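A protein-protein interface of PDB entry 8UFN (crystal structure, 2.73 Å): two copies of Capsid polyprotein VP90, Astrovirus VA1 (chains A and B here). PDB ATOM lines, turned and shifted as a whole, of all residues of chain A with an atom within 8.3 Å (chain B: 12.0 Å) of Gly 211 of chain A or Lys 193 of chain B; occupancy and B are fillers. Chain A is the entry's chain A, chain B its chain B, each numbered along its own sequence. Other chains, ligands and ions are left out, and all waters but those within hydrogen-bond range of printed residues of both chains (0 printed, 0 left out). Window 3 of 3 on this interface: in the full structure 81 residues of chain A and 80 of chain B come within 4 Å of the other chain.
Hydrophobic or aromatic side chains of chain A within 4 Å of the printed part of chain B: Phe 204, Pro 207 and Leu 213.
Along chain A the printed residues that touch a printed residue of chain B span positions 40 to 213.
Of the 15 printed residues of chain B, 12 touch a printed residue of chain A.
Printed residues of chain B that touch a printed residue of chain A: Ala 182, Leu 184, Tyr 187, Thr 188, Thr 189, Ser 192, Lys 193, Ser 194, Ala 195, Ile 196, Gln 197 and Lys 198.
Among the printed residues, 24 pairs touch across the chains.
Among the printed residues, Asp or Glu carboxylates within 4 Å of a Lys or Arg side-chain nitrogen of the other chain: Glu 208 of chain A with Lys 198 of chain B (3.97 Å).
Gln 40 of chain A touches Lys 198 of chain B.
Gln 202 of chain A touches Thr 189 of chain B.
CD2 of Phe 204 of chain A touches O of Thr 188 of chain B (3.6 Å).
CD2 of Phe 204 of chain A touches C of Ser 192 of chain B, at 3.3 Å.
CB of Ala 182 of chain B touches CE of Lys 206 of chain A (3.8 Å).
Lys 206 of chain A touches Leu 184 of chain B.
Pro 207 of chain A touches Lys 193 of chain B (CG to CG, 3.5 Å).
CA of Ala 195 of chain B touches O of Pro 207 of chain A (3.2 Å).
Gln 197 of chain B touches Glu 208 of chain A (OE1 to OE2, 3.9 Å).
Lys 193 of chain B touches Gly 211 of chain A.
The side-chain hydroxyl (OH) of Tyr 187 of chain B is in hydrogen-bond range of the side-chain amide oxygen (OE1) of Gln 202 of chain A, at 2.9 Å.
O of Pro 207 of chain A lies within hydrogen-bond range of N of Ile 196 of chain B, at 2.8 Å.
The backbone carbonyl oxygen of Ser 194 of chain B sits close to the backbone carbonyl oxygen of Pro 207 of chain A (3.2 Å).
The backbone carbonyl oxygen of Ser 192 of chain B lies within hydrogen-bond range of the backbone NH of Gln 205 of chain A, at 3.0 Å.
The backbone carbonyl oxygen (O) of Gln 205 of chain A lies within hydrogen-bond range of the backbone NH (N) of Ser 194 of chain B.
NZ of Lys 198 of chain B is in salt-bridge range of OE1 of Glu 208 of chain A (3.97 Å).
No position is printed for both chains.
N of Leu 181 of chain A sits at hydrogen-bond distance from O of Gln 202 of chain A (2.9 Å).
The backbone carbonyl oxygen (O) of Val 175 of chain A sits at hydrogen-bond distance from the backbone NH (N) of Leu 213 of chain A.
The backbone NH (N) of Gln 197 of chain B lies within hydrogen-bond range of the backbone carbonyl oxygen (O) of Tyr 183 of chain B.
OG1 of Thr 188 of chain B lies within hydrogen-bond range of N of Lys 193 of chain B (2.7 Å).
The backbone carbonyl oxygen (O) of Gln 177 of chain A lies within hydrogen-bond range of the backbone NH (N) of Lys 206 of chain A, 3.4 Å away.
OE1 of Gln 197 of chain B lies close to O of Ala 195 of chain B, at 3.2 Å.
No residue of chain B comes within 4 Å of Val 176 of chain A.
Of chain B, only Leu 184, Thr 188, Ser 192, Lys 193 and Ser 194 come within 4 Å of Phe 204 of chain A.
Of chain B, only Ser 192, Lys 193 and Ser 194 come within 4 Å of Gln 205 of chain A.
Printed residues of chain B within 4 Å of Lys 206 of chain A: Ala 182, Leu 184, Ser 194 and Ile 196.
Of chain B, only Lys 193 (3.5 Å), Ser 194 (3.1 Å), Ala 195 (3.2 Å) and Ile 196 (2.8 Å) come within 4 Å of Pro 207 of chain A.
Of chain B, only Lys 193 (3.6 Å) comes within 4 Å of Gly 211 of chain A.
No residue of chain B comes within 4 Å of Thr 212 of chain A.
Of the printed residues of chain A, Ala 182 of chain B touches Lys 206.
Thr 188 of chain B touches one residue of chain A.
Of chain A, only Phe 204, Gln 205, Pro 207 and Gly 211 come within 4 Å of Lys 193 of chain B.
Printed residues of chain A within 4 Å of Gln 197 of chain B: Glu 208 (3.9 Å).
The nearest residue of chain A that does not touch Lys 193 of chain B is Val 176 of chain A (5.1 Å).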
ATOM      1  N   GLN A  40      18.022 -24.738  20.464  1.00  0.00           N
ATOM      2  CA  GLN A  40      16.730 -24.690  19.798  1.00  0.00           C
ATOM      3  C   GLN A  40      15.771 -25.602  20.553  1.00  0.00           C
ATOM      4  O   GLN A  40      16.180 -26.625  21.107  1.00  0.00           O
ATOM      5  CB  GLN A  40      16.854 -25.107  18.324  1.00  0.00           C
ATOM      6  CG  GLN A  40      15.581 -25.647  17.685  1.00  0.00           C
ATOM      7  CD  GLN A  40      15.575 -25.484  16.177  1.00  0.00           C
ATOM      8  OE1 GLN A  40      15.598 -24.366  15.663  1.00  0.00           O
ATOM      9  NE2 GLN A  40      15.540 -26.603  15.461  1.00  0.00           N
ATOM     10  N   ASP A 174      14.741 -17.013  22.169  1.00  0.00           N
ATOM     11  CA  ASP A 174      15.435 -17.030  20.883  1.00  0.00           C
ATOM     12  C   ASP A 174      15.703 -15.604  20.414  1.00  0.00           C
ATOM     13  O   ASP A 174      14.764 -14.814  20.268  1.00  0.00           O
ATOM     14  CB  ASP A 174      14.607 -17.764  19.828  1.00  0.00           C
ATOM     15  CG  ASP A 174      14.319 -19.198  20.202  1.00  0.00           C
ATOM     16  OD1 ASP A 174      13.768 -19.420  21.298  1.00  0.00           O
ATOM     17  OD2 ASP A 174      14.633 -20.099  19.397  1.00  0.00           O
ATOM     18  N   VAL A 175      16.976 -15.282  20.164  1.00  0.00           N
ATOM     19  CA  VAL A 175      17.374 -14.004  19.577  1.00  0.00           C
ATOM     20  C   VAL A 175      18.563 -14.201  18.645  1.00  0.00           C
ATOM     21  O   VAL A 175      19.137 -15.285  18.532  1.00  0.00           O
ATOM     22  CB  VAL A 175      17.743 -12.927  20.623  1.00  0.00           C
ATOM     23  CG1 VAL A 175      16.667 -12.766  21.661  1.00  0.00           C
ATOM     24  CG2 VAL A 175      19.073 -13.278  21.273  1.00  0.00           C
ATOM     25  N   VAL A 176      18.917 -13.102  17.972  1.00  0.00           N
ATOM     26  CA  VAL A 176      20.171 -13.011  17.238  1.00  0.00           C
ATOM     27  C   VAL A 176      21.333 -13.236  18.194  1.00  0.00           C
ATOM     28  O   VAL A 176      21.455 -12.556  19.221  1.00  0.00           O
ATOM     29  CB  VAL A 176      20.263 -11.639  16.555  1.00  0.00           C
ATOM     30  CG1 VAL A 176      21.530 -11.525  15.742  1.00  0.00           C
ATOM     31  CG2 VAL A 176      19.033 -11.395  15.688  1.00  0.00           C
ATOM     32  N   GLN A 177      22.201 -14.191  17.858  1.00  0.00           N
ATOM     33  CA  GLN A 177      23.334 -14.551  18.704  1.00  0.00           C
ATOM     34  C   GLN A 177      24.621 -14.447  17.895  1.00  0.00           C
ATOM     35  O   GLN A 177      24.751 -15.078  16.840  1.00  0.00           O
ATOM     36  CB  GLN A 177      23.166 -15.961  19.275  1.00  0.00           C
ATOM     37  CG  GLN A 177      22.137 -16.047  20.397  1.00  0.00           C
ATOM     38  CD  GLN A 177      22.293 -17.297  21.244  1.00  0.00           C
ATOM     39  OE1 GLN A 177      23.304 -17.478  21.923  1.00  0.00           O
ATOM     40  NE2 GLN A 177      21.287 -18.162  21.213  1.00  0.00           N
ATOM     41  N   LEU A 181      34.439 -17.107  14.942  1.00  0.00           N
ATOM     42  CA  LEU A 181      34.899 -18.187  14.070  1.00  0.00           C
ATOM     43  C   LEU A 181      35.963 -17.617  13.134  1.00  0.00           C
ATOM     44  O   LEU A 181      36.383 -16.463  13.275  1.00  0.00           O
ATOM     45  CB  LEU A 181      33.730 -18.812  13.303  1.00  0.00           C
ATOM     46  CG  LEU A 181      33.243 -18.108  12.030  1.00  0.00           C
ATOM     47  CD1 LEU A 181      32.331 -19.016  11.216  1.00  0.00           C
ATOM     48  CD2 LEU A 181      32.551 -16.790  12.338  1.00  0.00           C
ATOM     49  N   GLN A 202      36.546 -13.414  11.995  1.00  0.00           N
ATOM     50  CA  GLN A 202      35.149 -13.205  11.642  1.00  0.00           C
ATOM     51  C   GLN A 202      34.245 -13.558  12.815  1.00  0.00           C
ATOM     52  O   GLN A 202      34.480 -14.538  13.531  1.00  0.00           O
ATOM     53  CB  GLN A 202      34.749 -14.029  10.413  1.00  0.00           C
ATOM     54  CG  GLN A 202      33.413 -13.606   9.803  1.00  0.00           C
ATOM     55  CD  GLN A 202      32.672 -14.752   9.143  1.00  0.00           C
ATOM     56  OE1 GLN A 202      33.244 -15.807   8.883  1.00  0.00           O
ATOM     57  NE2 GLN A 202      31.389 -14.545   8.865  1.00  0.00           N
ATOM     58  N   THR A 203      33.209 -12.744  13.006  1.00  0.00           N
ATOM     59  CA  THR A 203      32.194 -12.952  14.034  1.00  0.00           C
ATOM     60  C   THR A 203      30.846 -12.657  13.402  1.00  0.00           C
ATOM     61  O   THR A 203      30.552 -11.502  13.085  1.00  0.00           O
ATOM     62  CB  THR A 203      32.420 -12.053  15.244  1.00  0.00           C
ATOM     63  OG1 THR A 203      33.765 -12.207  15.710  1.00  0.00           O
ATOM     64  CG2 THR A 203      31.470 -12.430  16.354  1.00  0.00           C
ATOM     65  N   PHE A 204      30.027 -13.687  13.223  1.00  0.00           N
ATOM     66  CA  PHE A 204      28.784 -13.542  12.476  1.00  0.00           C
ATOM     67  C   PHE A 204      27.626 -14.114  13.291  1.00  0.00           C
ATOM     68  O   PHE A 204      27.696 -14.265  14.519  1.00  0.00           O
ATOM     69  CB  PHE A 204      28.941 -14.165  11.074  1.00  0.00           C
ATOM     70  CG  PHE A 204      28.836 -15.680  11.021  1.00  0.00           C
ATOM     71  CD1 PHE A 204      29.495 -16.507  11.926  1.00  0.00           C
ATOM     72  CD2 PHE A 204      28.067 -16.274  10.037  1.00  0.00           C
ATOM     73  CE1 PHE A 204      29.376 -17.887  11.842  1.00  0.00           C
ATOM     74  CE2 PHE A 204      27.945 -17.647   9.950  1.00  0.00           C
ATOM     75  CZ  PHE A 204      28.597 -18.455  10.851  1.00  0.00           C
ATOM     76  N   GLN A 205      26.538 -14.441  12.600  1.00  0.00           N
ATOM     77  CA  GLN A 205      25.308 -14.911  13.216  1.00  0.00           C
ATOM     78  C   GLN A 205      25.194 -16.422  13.095  1.00  0.00           C
ATOM     79  O   GLN A 205      25.586 -17.007  12.080  1.00  0.00           O
ATOM     80  CB  GLN A 205      24.092 -14.259  12.561  1.00  0.00           C
ATOM     81  CG  GLN A 205      23.461 -13.172  13.386  1.00  0.00           C
ATOM     82  CD  GLN A 205      24.464 -12.143  13.855  1.00  0.00           C
ATOM     83  OE1 GLN A 205      24.681 -11.973  15.053  1.00  0.00           O
ATOM     84  NE2 GLN A 205      25.072 -11.433  12.911  1.00  0.00           N
ATOM     85  N   LYS A 206      24.646 -17.050  14.132  1.00  0.00           N
ATOM     86  CA  LYS A 206      24.447 -18.497  14.171  1.00  0.00           C
ATOM     87  C   LYS A 206      23.010 -18.794  14.582  1.00  0.00           C
ATOM     88  O   LYS A 206      22.740 -19.119  15.745  1.00  0.00           O
ATOM     89  CB  LYS A 206      25.445 -19.162  15.121  1.00  0.00           C
ATOM     90  CG  LYS A 206      26.798 -19.457  14.494  1.00  0.00           C
ATOM     91  CD  LYS A 206      27.559 -20.509  15.287  1.00  0.00           C
ATOM     92  CE  LYS A 206      28.885 -20.849  14.626  1.00  0.00           C
ATOM     93  NZ  LYS A 206      29.860 -19.727  14.702  1.00  0.00           N
ATOM     94  N   PRO A 207      22.056 -18.684  13.652  1.00  0.00           N
ATOM     95  CA  PRO A 207      20.685 -19.108  13.952  1.00  0.00           C
ATOM     96  C   PRO A 207      20.392 -20.511  13.449  1.00  0.00           C
ATOM     97  O   PRO A 207      21.251 -21.144  12.827  1.00  0.00           O
ATOM     98  CB  PRO A 207      19.843 -18.067  13.213  1.00  0.00           C
ATOM     99  CG  PRO A 207      20.652 -17.793  11.988  1.00  0.00           C
ATOM    100  CD  PRO A 207      22.115 -17.918  12.394  1.00  0.00           C
ATOM    101  N   GLU A 208      19.180 -21.005  13.693  1.00  0.00           N
ATOM    102  CA  GLU A 208      18.771 -22.314  13.202  1.00  0.00           C
ATOM    103  C   GLU A 208      17.311 -22.272  12.788  1.00  0.00           C
ATOM    104  O   GLU A 208      16.465 -21.770  13.532  1.00  0.00           O
ATOM    105  CB  GLU A 208      18.983 -23.397  14.263  1.00  0.00           C
ATOM    106  CG  GLU A 208      19.372 -24.752  13.689  1.00  0.00           C
ATOM    107  CD  GLU A 208      18.311 -25.354  12.793  1.00  0.00           C
ATOM    108  OE1 GLU A 208      17.173 -25.546  13.268  1.00  0.00           O
ATOM    109  OE2 GLU A 208      18.617 -25.648  11.620  1.00  0.00           O
ATOM    110  N   GLY A 209      17.023 -22.810  11.607  1.00  0.00           N
ATOM    111  CA  GLY A 209      15.665 -22.856  11.105  1.00  0.00           C
ATOM    112  C   GLY A 209      15.141 -21.496  10.699  1.00  0.00           C
ATOM    113  O   GLY A 209      14.968 -21.219   9.508  1.00  0.00           O
ATOM    114  N   GLY A 210      14.884 -20.637  11.681  1.00  0.00           N
ATOM    115  CA  GLY A 210      14.378 -19.306  11.410  1.00  0.00           C
ATOM    116  C   GLY A 210      15.475 -18.287  11.182  1.00  0.00           C
ATOM    117  O   GLY A 210      16.303 -18.444  10.279  1.00  0.00           O
ATOM    118  N   GLY A 211      15.490 -17.235  11.996  1.00  0.00           N
ATOM    119  CA  GLY A 211      16.505 -16.207  11.873  1.00  0.00           C
ATOM    120  C   GLY A 211      17.231 -15.930  13.173  1.00  0.00           C
ATOM    121  O   GLY A 211      18.138 -15.094  13.217  1.00  0.00           O
ATOM    122  N   THR A 212      16.847 -16.631  14.237  1.00  0.00           N
ATOM    123  CA  THR A 212      17.409 -16.430  15.565  1.00  0.00           C
ATOM    124  C   THR A 212      17.846 -17.773  16.144  1.00  0.00           C
ATOM    125  O   THR A 212      17.726 -18.822  15.507  1.00  0.00           O
ATOM    126  CB  THR A 212      16.399 -15.746  16.496  1.00  0.00           C
ATOM    127  OG1 THR A 212      15.203 -16.532  16.572  1.00  0.00           O
ATOM    128  CG2 THR A 212      16.058 -14.352  15.989  1.00  0.00           C
ATOM    129  N   LEU A 213      18.355 -17.728  17.375  1.00  0.00           N
ATOM    130  CA  LEU A 213      18.812 -18.913  18.083  1.00  0.00           C
ATOM    131  C   LEU A 213      18.434 -18.798  19.552  1.00  0.00           C
ATOM    132  O   LEU A 213      18.483 -17.709  20.128  1.00  0.00           O
ATOM    133  CB  LEU A 213      20.329 -19.097  17.945  1.00  0.00           C
ATOM    134  CG  LEU A 213      20.888 -20.464  18.336  1.00  0.00           C
ATOM    135  CD1 LEU A 213      20.672 -21.480  17.225  1.00  0.00           C
ATOM    136  CD2 LEU A 213      22.360 -20.342  18.680  1.00  0.00           C
ATOM    137  N   ARG A 214      18.068 -19.928  20.154  1.00  0.00           N
ATOM    138  CA  ARG A 214      17.605 -19.939  21.535  1.00  0.00           C
ATOM    139  C   ARG A 214      18.781 -19.988  22.504  1.00  0.00           C
ATOM    140  O   ARG A 214      19.752 -20.720  22.291  1.00  0.00           O
ATOM    141  CB  ARG A 214      16.677 -21.130  21.778  1.00  0.00           C
ATOM    142  CG  ARG A 214      16.560 -21.546  23.236  1.00  0.00           C
ATOM    143  CD  ARG A 214      15.188 -22.116  23.549  1.00  0.00           C
ATOM    144  NE  ARG A 214      14.117 -21.214  23.142  1.00  0.00           N
ATOM    145  CZ  ARG A 214      12.841 -21.563  23.050  1.00  0.00           C
ATOM    146  NH1 ARG A 214      12.432 -22.780  23.365  1.00  0.00           N
ATOM    147  NH2 ARG A 214      11.952 -20.665  22.633  1.00  0.00           N
ATOM    148  N   ALA B 182      32.246 -25.329  14.151  1.00  0.00           N
ATOM    149  CA  ALA B 182      30.848 -25.692  14.304  1.00  0.00           C
ATOM    150  C   ALA B 182      30.287 -26.191  12.979  1.00  0.00           C
ATOM    151  O   ALA B 182      30.767 -25.820  11.903  1.00  0.00           O
ATOM    152  CB  ALA B 182      30.038 -24.492  14.796  1.00  0.00           C
ATOM    153  N   TYR B 183      29.262 -27.036  13.062  1.00  0.00           N
ATOM    154  CA  TYR B 183      28.629 -27.598  11.870  1.00  0.00           C
ATOM    155  C   TYR B 183      27.625 -26.588  11.331  1.00  0.00           C
ATOM    156  O   TYR B 183      26.502 -26.479  11.827  1.00  0.00           O
ATOM    157  CB  TYR B 183      27.957 -28.929  12.190  1.00  0.00           C
ATOM    158  CG  TYR B 183      27.628 -29.762  10.970  1.00  0.00           C
ATOM    159  CD1 TYR B 183      28.609 -30.485  10.305  1.00  0.00           C
ATOM    160  CD2 TYR B 183      26.337 -29.817  10.476  1.00  0.00           C
ATOM    161  CE1 TYR B 183      28.299 -31.249   9.192  1.00  0.00           C
ATOM    162  CE2 TYR B 183      26.018 -30.567   9.368  1.00  0.00           C
ATOM    163  CZ  TYR B 183      27.002 -31.281   8.727  1.00  0.00           C
ATOM    164  OH  TYR B 183      26.682 -32.030   7.619  1.00  0.00           O
ATOM    165  N   LEU B 184      28.031 -25.842  10.309  1.00  0.00           N
ATOM    166  CA  LEU B 184      27.172 -24.870   9.651  1.00  0.00           C
ATOM    167  C   LEU B 184      26.610 -25.473   8.369  1.00  0.00           C
ATOM    168  O   LEU B 184      27.255 -26.299   7.717  1.00  0.00           O
ATOM    169  CB  LEU B 184      27.945 -23.586   9.341  1.00  0.00           C
ATOM    170  CG  LEU B 184      28.907 -23.111  10.436  1.00  0.00           C
ATOM    171  CD1 LEU B 184      29.555 -21.790  10.060  1.00  0.00           C
ATOM    172  CD2 LEU B 184      28.195 -22.985  11.777  1.00  0.00           C
ATOM    173  N   GLU B 185      25.394 -25.060   8.012  1.00  0.00           N
ATOM    174  CA  GLU B 185      24.689 -25.663   6.890  1.00  0.00           C
ATOM    175  C   GLU B 185      24.309 -24.682   5.791  1.00  0.00           C
ATOM    176  O   GLU B 185      24.265 -25.080   4.625  1.00  0.00           O
ATOM    177  CB  GLU B 185      23.419 -26.375   7.382  1.00  0.00           C
ATOM    178  CG  GLU B 185      23.023 -27.574   6.540  1.00  0.00           C
ATOM    179  CD  GLU B 185      23.631 -28.868   7.051  1.00  0.00           C
ATOM    180  OE1 GLU B 185      23.311 -29.268   8.190  1.00  0.00           O
ATOM    181  OE2 GLU B 185      24.429 -29.483   6.313  1.00  0.00           O
ATOM    182  N   ASP B 186      24.034 -23.426   6.121  1.00  0.00           N
ATOM    183  CA  ASP B 186      23.703 -22.395   5.139  1.00  0.00           C
ATOM    184  C   ASP B 186      24.688 -21.242   5.306  1.00  0.00           C
ATOM    185  O   ASP B 186      24.303 -20.127   5.670  1.00  0.00           O
ATOM    186  CB  ASP B 186      22.245 -21.924   5.307  1.00  0.00           C
ATOM    187  CG  ASP B 186      21.236 -22.965   4.857  1.00  0.00           C
ATOM    188  OD1 ASP B 186      21.653 -24.017   4.330  1.00  0.00           O
ATOM    189  OD2 ASP B 186      20.022 -22.728   5.033  1.00  0.00           O
ATOM    190  N   TYR B 187      25.961 -21.511   5.027  1.00  0.00           N
ATOM    191  CA  TYR B 187      27.014 -20.565   5.370  1.00  0.00           C
ATOM    192  C   TYR B 187      26.961 -19.319   4.498  1.00  0.00           C
ATOM    193  O   TYR B 187      26.774 -19.394   3.280  1.00  0.00           O
ATOM    194  CB  TYR B 187      28.388 -21.216   5.241  1.00  0.00           C
ATOM    195  CG  TYR B 187      29.507 -20.288   5.657  1.00  0.00           C
ATOM    196  CD1 TYR B 187      29.774 -20.052   6.999  1.00  0.00           C
ATOM    197  CD2 TYR B 187      30.277 -19.626   4.711  1.00  0.00           C
ATOM    198  CE1 TYR B 187      30.786 -19.198   7.387  1.00  0.00           C
ATOM    199  CE2 TYR B 187      31.292 -18.771   5.089  1.00  0.00           C
ATOM    200  CZ  TYR B 187      31.543 -18.560   6.428  1.00  0.00           C
ATOM    201  OH  TYR B 187      32.551 -17.707   6.812  1.00  0.00           O
ATOM    202  N   THR B 188      27.132 -18.162   5.138  1.00  0.00           N
ATOM    203  CA  THR B 188      27.307 -16.888   4.459  1.00  0.00           C
ATOM    204  C   THR B 188      28.338 -16.061   5.211  1.00  0.00           C
ATOM    205  O   THR B 188      28.332 -16.019   6.445  1.00  0.00           O
ATOM    206  CB  THR B 188      26.001 -16.078   4.370  1.00  0.00           C
ATOM    207  OG1 THR B 188      25.541 -15.759   5.691  1.00  0.00           O
ATOM    208  CG2 THR B 188      24.916 -16.841   3.621  1.00  0.00           C
ATOM    209  N   THR B 189      29.225 -15.408   4.462  1.00  0.00           N
ATOM    210  CA  THR B 189      30.042 -14.333   4.997  1.00  0.00           C
ATOM    211  C   THR B 189      29.777 -13.001   4.316  1.00  0.00           C
ATOM    212  O   THR B 189      30.275 -11.973   4.787  1.00  0.00           O
ATOM    213  CB  THR B 189      31.539 -14.663   4.877  1.00  0.00           C
ATOM    214  OG1 THR B 189      32.304 -13.478   5.129  1.00  0.00           O
ATOM    215  CG2 THR B 189      31.861 -15.177   3.483  1.00  0.00           C
ATOM    216  N   SER B 192      27.159 -13.550   6.497  1.00  0.00           N
ATOM    217  CA  SER B 192      27.252 -13.131   7.889  1.00  0.00           C
ATOM    218  C   SER B 192      26.245 -13.883   8.752  1.00  0.00           C
ATOM    219  O   SER B 192      25.876 -13.423   9.834  1.00  0.00           O
ATOM    220  CB  SER B 192      27.030 -11.620   8.005  1.00  0.00           C
ATOM    221  OG  SER B 192      26.416 -11.285   9.237  1.00  0.00           O
ATOM    222  N   LYS B 193      25.808 -15.046   8.271  1.00  0.00           N
ATOM    223  CA  LYS B 193      24.789 -15.829   8.955  1.00  0.00           C
ATOM    224  C   LYS B 193      24.791 -17.243   8.387  1.00  0.00           C
ATOM    225  O   LYS B 193      24.985 -17.429   7.183  1.00  0.00           O
ATOM    226  CB  LYS B 193      23.405 -15.186   8.799  1.00  0.00           C
ATOM    227  CG  LYS B 193      22.266 -15.976   9.417  1.00  0.00           C
ATOM    228  CD  LYS B 193      20.958 -15.201   9.381  1.00  0.00           C
ATOM    229  CE  LYS B 193      21.155 -13.757   9.822  1.00  0.00           C
ATOM    230  NZ  LYS B 193      20.583 -13.499  11.172  1.00  0.00           N
ATOM    231  N   SER B 194      24.579 -18.229   9.256  1.00  0.00           N
ATOM    232  CA  SER B 194      24.559 -19.622   8.830  1.00  0.00           C
ATOM    233  C   SER B 194      23.733 -20.445   9.807  1.00  0.00           C
ATOM    234  O   SER B 194      23.729 -20.185  11.013  1.00  0.00           O
ATOM    235  CB  SER B 194      25.973 -20.202   8.727  1.00  0.00           C
ATOM    236  OG  SER B 194      26.437 -20.646   9.990  1.00  0.00           O
ATOM    237  N   ALA B 195      23.042 -21.450   9.273  1.00  0.00           N
ATOM    238  CA  ALA B 195      22.275 -22.368  10.107  1.00  0.00           C
ATOM    239  C   ALA B 195      23.224 -23.254  10.903  1.00  0.00           C
ATOM    240  O   ALA B 195      23.988 -24.034  10.322  1.00  0.00           O
ATOM    241  CB  ALA B 195      21.340 -23.213   9.246  1.00  0.00           C
ATOM    242  N   ILE B 196      23.178 -23.137  12.225  1.00  0.00           N
ATOM    243  CA  ILE B 196      24.113 -23.824  13.111  1.00  0.00           C
ATOM    244  C   ILE B 196      23.429 -25.038  13.718  1.00  0.00           C
ATOM    245  O   ILE B 196      22.319 -24.934  14.254  1.00  0.00           O
ATOM    246  CB  ILE B 196      24.629 -22.886  14.214  1.00  0.00           C
ATOM    247  CG1 ILE B 196      25.314 -23.705  15.296  1.00  0.00           C
ATOM    248  CG2 ILE B 196      23.484 -22.122  14.837  1.00  0.00           C
ATOM    249  CD1 ILE B 196      26.617 -24.283  14.871  1.00  0.00           C
ATOM    250  N   GLN B 197      24.094 -26.185  13.658  1.00  0.00           N
ATOM    251  CA  GLN B 197      23.580 -27.400  14.268  1.00  0.00           C
ATOM    252  C   GLN B 197      24.121 -27.526  15.685  1.00  0.00           C
ATOM    253  O   GLN B 197      25.341 -27.505  15.896  1.00  0.00           O
ATOM    254  CB  GLN B 197      23.953 -28.624  13.439  1.00  0.00           C
ATOM    255  CG  GLN B 197      23.861 -28.392  11.949  1.00  0.00           C
ATOM    256  CD  GLN B 197      22.508 -27.882  11.510  1.00  0.00           C
ATOM    257  OE1 GLN B 197      22.360 -26.716  11.147  1.00  0.00           O
ATOM    258  NE2 GLN B 197      21.509 -28.758  11.535  1.00  0.00           N
ATOM    259  N   LYS B 198      23.215 -27.642  16.647  1.00  0.00           N
ATOM    260  CA  LYS B 198      23.591 -27.945  18.016  1.00  0.00           C
ATOM    261  C   LYS B 198      23.841 -29.444  18.146  1.00  0.00           C
ATOM    262  O   LYS B 198      23.625 -30.220  17.210  1.00  0.00           O
ATOM    263  CB  LYS B 198      22.513 -27.483  19.002  1.00  0.00           C
ATOM    264  CG  LYS B 198      22.165 -25.989  18.954  1.00  0.00           C
ATOM    265  CD  LYS B 198      21.417 -25.603  17.693  1.00  0.00           C
ATOM    266  CE  LYS B 198      20.184 -26.462  17.545  1.00  0.00           C
ATOM    267  NZ  LYS B 198      19.720 -26.534  16.143  1.00  0.00           N
